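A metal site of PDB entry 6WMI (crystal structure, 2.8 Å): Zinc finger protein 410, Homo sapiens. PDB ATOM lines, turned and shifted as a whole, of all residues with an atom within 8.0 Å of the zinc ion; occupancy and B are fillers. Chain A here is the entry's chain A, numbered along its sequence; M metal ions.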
ATOM      1  N   LYS A   9       4.483  14.462  13.391  1.00  0.00           N
ATOM      2  CA  LYS A   9       3.653  13.277  13.516  1.00  0.00           C
ATOM      3  C   LYS A   9       4.092  12.521  14.763  1.00  0.00           C
ATOM      4  O   LYS A   9       5.294  12.308  14.967  1.00  0.00           O
ATOM      5  CB  LYS A   9       3.755  12.373  12.292  1.00  0.00           C
ATOM      6  N   CYS A  10       3.138  12.129  15.605  1.00  0.00           N
ATOM      7  CA  CYS A  10       3.456  11.336  16.784  1.00  0.00           C
ATOM      8  C   CYS A  10       3.961   9.972  16.354  1.00  0.00           C
ATOM      9  O   CYS A  10       3.372   9.326  15.479  1.00  0.00           O
ATOM     10  CB  CYS A  10       2.257  11.180  17.703  1.00  0.00           C
ATOM     11  SG  CYS A  10       2.632  10.239  19.200  1.00  0.00           S
ATOM     12  N   THR A  11       5.032   9.520  16.985  1.00  0.00           N
ATOM     13  CA  THR A  11       5.741   8.323  16.561  1.00  0.00           C
ATOM     14  C   THR A  11       5.610   7.179  17.563  1.00  0.00           C
ATOM     15  O   THR A  11       6.249   6.134  17.373  1.00  0.00           O
ATOM     16  CB  THR A  11       7.208   8.661  16.315  1.00  0.00           C
ATOM     17  OG1 THR A  11       7.741   9.328  17.474  1.00  0.00           O
ATOM     18  CG2 THR A  11       7.338   9.591  15.121  1.00  0.00           C
ATOM     19  N   VAL A  12       4.814   7.354  18.622  1.00  0.00           N
ATOM     20  CA  VAL A  12       4.520   6.244  19.529  1.00  0.00           C
ATOM     21  C   VAL A  12       3.762   5.165  18.745  1.00  0.00           C
ATOM     22  O   VAL A  12       3.162   5.408  17.691  1.00  0.00           O
ATOM     23  CB  VAL A  12       3.714   6.736  20.747  1.00  0.00           C
ATOM     24  CG1 VAL A  12       3.529   5.633  21.784  1.00  0.00           C
ATOM     25  CG2 VAL A  12       4.419   7.908  21.384  1.00  0.00           C
ATOM     26  N   GLU A  13       3.792   3.946  19.293  1.00  0.00           N
ATOM     27  CA  GLU A  13       3.485   2.744  18.514  1.00  0.00           C
ATOM     28  C   GLU A  13       2.105   2.807  17.861  1.00  0.00           C
ATOM     29  O   GLU A  13       1.985   2.787  16.638  1.00  0.00           O
ATOM     30  CB  GLU A  13       3.607   1.509  19.413  1.00  0.00           C
ATOM     31  CG  GLU A  13       3.191   0.207  18.727  1.00  0.00           C
ATOM     32  CD  GLU A  13       3.819   0.029  17.350  1.00  0.00           C
ATOM     33  OE1 GLU A  13       4.993   0.424  17.161  1.00  0.00           O
ATOM     34  OE2 GLU A  13       3.139  -0.506  16.459  1.00  0.00           O
ATOM     35  N   GLY A  14       1.057   2.874  18.669  1.00  0.00           N
ATOM     36  CA  GLY A  14      -0.290   2.806  18.124  1.00  0.00           C
ATOM     37  C   GLY A  14      -0.966   4.121  17.846  1.00  0.00           C
ATOM     38  O   GLY A  14      -2.176   4.133  17.587  1.00  0.00           O
ATOM     39  N   CYS A  15      -0.234   5.242  17.866  1.00  0.00           N
ATOM     40  CA  CYS A  15      -0.894   6.554  17.839  1.00  0.00           C
ATOM     41  C   CYS A  15      -1.247   7.006  16.412  1.00  0.00           C
ATOM     42  O   CYS A  15      -2.421   7.121  16.066  1.00  0.00           O
ATOM     43  CB  CYS A  15      -0.007   7.585  18.529  1.00  0.00           C
ATOM     44  SG  CYS A  15      -0.806   9.174  18.818  1.00  0.00           S
ATOM     45  N   ASP A  16      -0.222   7.235  15.581  1.00  0.00           N
ATOM     46  CA  ASP A  16      -0.405   7.716  14.211  1.00  0.00           C
ATOM     47  C   ASP A  16      -1.299   8.955  14.163  1.00  0.00           C
ATOM     48  O   ASP A  16      -2.372   8.962  13.544  1.00  0.00           O
ATOM     49  CB  ASP A  16      -0.953   6.615  13.297  1.00  0.00           C
ATOM     50  CG  ASP A  16      -0.005   5.422  13.163  1.00  0.00           C
ATOM     51  OD1 ASP A  16      -0.159   4.436  13.911  1.00  0.00           O
ATOM     52  OD2 ASP A  16       0.880   5.472  12.282  1.00  0.00           O
ATOM     53  N   ARG A  17      -0.856  10.021  14.826  1.00  0.00           N
ATOM     54  CA  ARG A  17      -1.554  11.303  14.836  1.00  0.00           C
ATOM     55  C   ARG A  17      -0.601  12.413  14.425  1.00  0.00           C
ATOM     56  O   ARG A  17       0.600  12.343  14.700  1.00  0.00           O
ATOM     57  CB  ARG A  17      -2.153  11.646  16.209  1.00  0.00           C
ATOM     58  CG  ARG A  17      -3.415  10.883  16.570  1.00  0.00           C
ATOM     59  CD  ARG A  17      -4.089  11.498  17.790  1.00  0.00           C
ATOM     60  NE  ARG A  17      -4.408  12.904  17.573  1.00  0.00           N
ATOM     61  CZ  ARG A  17      -4.889  13.718  18.509  1.00  0.00           C
ATOM     62  NH1 ARG A  17      -5.106  13.266  19.737  1.00  0.00           N
ATOM     63  NH2 ARG A  17      -5.142  14.990  18.214  1.00  0.00           N
ATOM     64  N   THR A  18      -1.141  13.434  13.773  1.00  0.00           N
ATOM     65  CA  THR A  18      -0.327  14.515  13.233  1.00  0.00           C
ATOM     66  C   THR A  18      -0.869  15.850  13.710  1.00  0.00           C
ATOM     67  O   THR A  18      -2.080  16.037  13.864  1.00  0.00           O
ATOM     68  CB  THR A  18      -0.282  14.455  11.705  1.00  0.00           C
ATOM     69  OG1 THR A  18       0.364  15.621  11.196  1.00  0.00           O
ATOM     70  CG2 THR A  18      -1.699  14.333  11.126  1.00  0.00           C
ATOM     71  N   PHE A  19       0.044  16.792  13.940  1.00  0.00           N
ATOM     72  CA  PHE A  19      -0.272  18.048  14.604  1.00  0.00           C
ATOM     73  C   PHE A  19       0.188  19.226  13.767  1.00  0.00           C
ATOM     74  O   PHE A  19       0.923  19.085  12.789  1.00  0.00           O
ATOM     75  CB  PHE A  19       0.372  18.099  16.010  1.00  0.00           C
ATOM     76  CG  PHE A  19      -0.155  17.049  16.937  1.00  0.00           C
ATOM     77  CD1 PHE A  19      -1.170  17.342  17.831  1.00  0.00           C
ATOM     78  CD2 PHE A  19       0.339  15.756  16.894  1.00  0.00           C
ATOM     79  CE1 PHE A  19      -1.668  16.377  18.679  1.00  0.00           C
ATOM     80  CE2 PHE A  19      -0.154  14.777  17.734  1.00  0.00           C
ATOM     81  CZ  PHE A  19      -1.173  15.091  18.623  1.00  0.00           C
ATOM     82  N   PHE A  25       1.728  19.753  20.008  1.00  0.00           N
ATOM     83  CA  PHE A  25       2.504  18.522  19.892  1.00  0.00           C
ATOM     84  C   PHE A  25       3.187  18.193  21.210  1.00  0.00           C
ATOM     85  O   PHE A  25       3.165  17.047  21.659  1.00  0.00           O
ATOM     86  CB  PHE A  25       3.525  18.659  18.767  1.00  0.00           C
ATOM     87  CG  PHE A  25       4.350  17.433  18.544  1.00  0.00           C
ATOM     88  CD1 PHE A  25       3.761  16.250  18.124  1.00  0.00           C
ATOM     89  CD2 PHE A  25       5.713  17.458  18.726  1.00  0.00           C
ATOM     90  CE1 PHE A  25       4.513  15.116  17.907  1.00  0.00           C
ATOM     91  CE2 PHE A  25       6.474  16.320  18.507  1.00  0.00           C
ATOM     92  CZ  PHE A  25       5.862  15.152  18.111  1.00  0.00           C
ATOM     93  N   HIS A  28       0.799  16.743  23.624  1.00  0.00           N
ATOM     94  CA  HIS A  28       0.435  15.361  23.324  1.00  0.00           C
ATOM     95  C   HIS A  28       1.488  14.384  23.842  1.00  0.00           C
ATOM     96  O   HIS A  28       1.157  13.344  24.413  1.00  0.00           O
ATOM     97  CB  HIS A  28       0.234  15.179  21.821  1.00  0.00           C
ATOM     98  CG  HIS A  28      -0.216  13.808  21.434  1.00  0.00           C
ATOM     99  ND1 HIS A  28      -1.480  13.324  21.739  1.00  0.00           N
ATOM    100  CD2 HIS A  28       0.412  12.813  20.770  1.00  0.00           C
ATOM    101  CE1 HIS A  28      -1.599  12.094  21.270  1.00  0.00           C
ATOM    102  NE2 HIS A  28      -0.467  11.760  20.674  1.00  0.00           N
ATOM    103  N   LEU A  29       2.767  14.713  23.654  1.00  0.00           N
ATOM    104  CA  LEU A  29       3.823  13.840  24.156  1.00  0.00           C
ATOM    105  C   LEU A  29       3.753  13.694  25.666  1.00  0.00           C
ATOM    106  O   LEU A  29       3.982  12.607  26.208  1.00  0.00           O
ATOM    107  CB  LEU A  29       5.197  14.380  23.726  1.00  0.00           C
ATOM    108  CG  LEU A  29       5.422  14.421  22.215  1.00  0.00           C
ATOM    109  CD1 LEU A  29       6.692  15.160  21.890  1.00  0.00           C
ATOM    110  CD2 LEU A  29       5.449  13.014  21.647  1.00  0.00           C
ATOM    111  N   THR A  31       1.133  13.697  27.546  1.00  0.00           N
ATOM    112  CA  THR A  31       0.069  12.784  27.947  1.00  0.00           C
ATOM    113  C   THR A  31       0.483  11.326  27.784  1.00  0.00           C
ATOM    114  O   THR A  31       0.039  10.475  28.559  1.00  0.00           O
ATOM    115  CB  THR A  31      -1.210  13.040  27.140  1.00  0.00           C
ATOM    116  OG1 THR A  31      -1.041  12.570  25.795  1.00  0.00           O
ATOM    117  CG2 THR A  31      -1.546  14.524  27.120  1.00  0.00           C
ATOM    118  N   HIS A  32       1.318  11.026  26.787  1.00  0.00           N
ATOM    119  CA  HIS A  32       1.823   9.662  26.632  1.00  0.00           C
ATOM    120  C   HIS A  32       2.709   9.274  27.799  1.00  0.00           C
ATOM    121  O   HIS A  32       2.719   8.110  28.222  1.00  0.00           O
ATOM    122  CB  HIS A  32       2.584   9.527  25.318  1.00  0.00           C
ATOM    123  CG  HIS A  32       1.702   9.299  24.118  1.00  0.00           C
ATOM    124  ND1 HIS A  32       0.960   8.156  23.947  1.00  0.00           N
ATOM    125  CD2 HIS A  32       1.466  10.072  23.029  1.00  0.00           C
ATOM    126  CE1 HIS A  32       0.287   8.233  22.814  1.00  0.00           C
ATOM    127  NE2 HIS A  32       0.582   9.382  22.235  1.00  0.00           N
HETATM  128 ZN    ZN M   1       0.577  10.010  20.333  1.00  0.00          ZN
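N of Cys 10 is in hydrogen-bond range of O of Arg 17, at 2.7 Å.
O of His 28 sits at hydrogen-bond distance from OG1 of Thr 31 (2.7 Å).
The side-chain sulfur (SG) of Cys 10 sits close to the backbone NH (N) of Val 12, 3.7 Å away.
The zinc ion is bound by a ring nitrogen (NE2) of His 32 (2.0 Å), a ring nitrogen (NE2) of His 28 (2.1 Å), the side-chain sulfur (SG) of Cys 15 (2.2 Å) and the side-chain sulfur (SG) of Cys 10 (2.4 Å).
The zinc ion has four donor atoms within binding distance.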
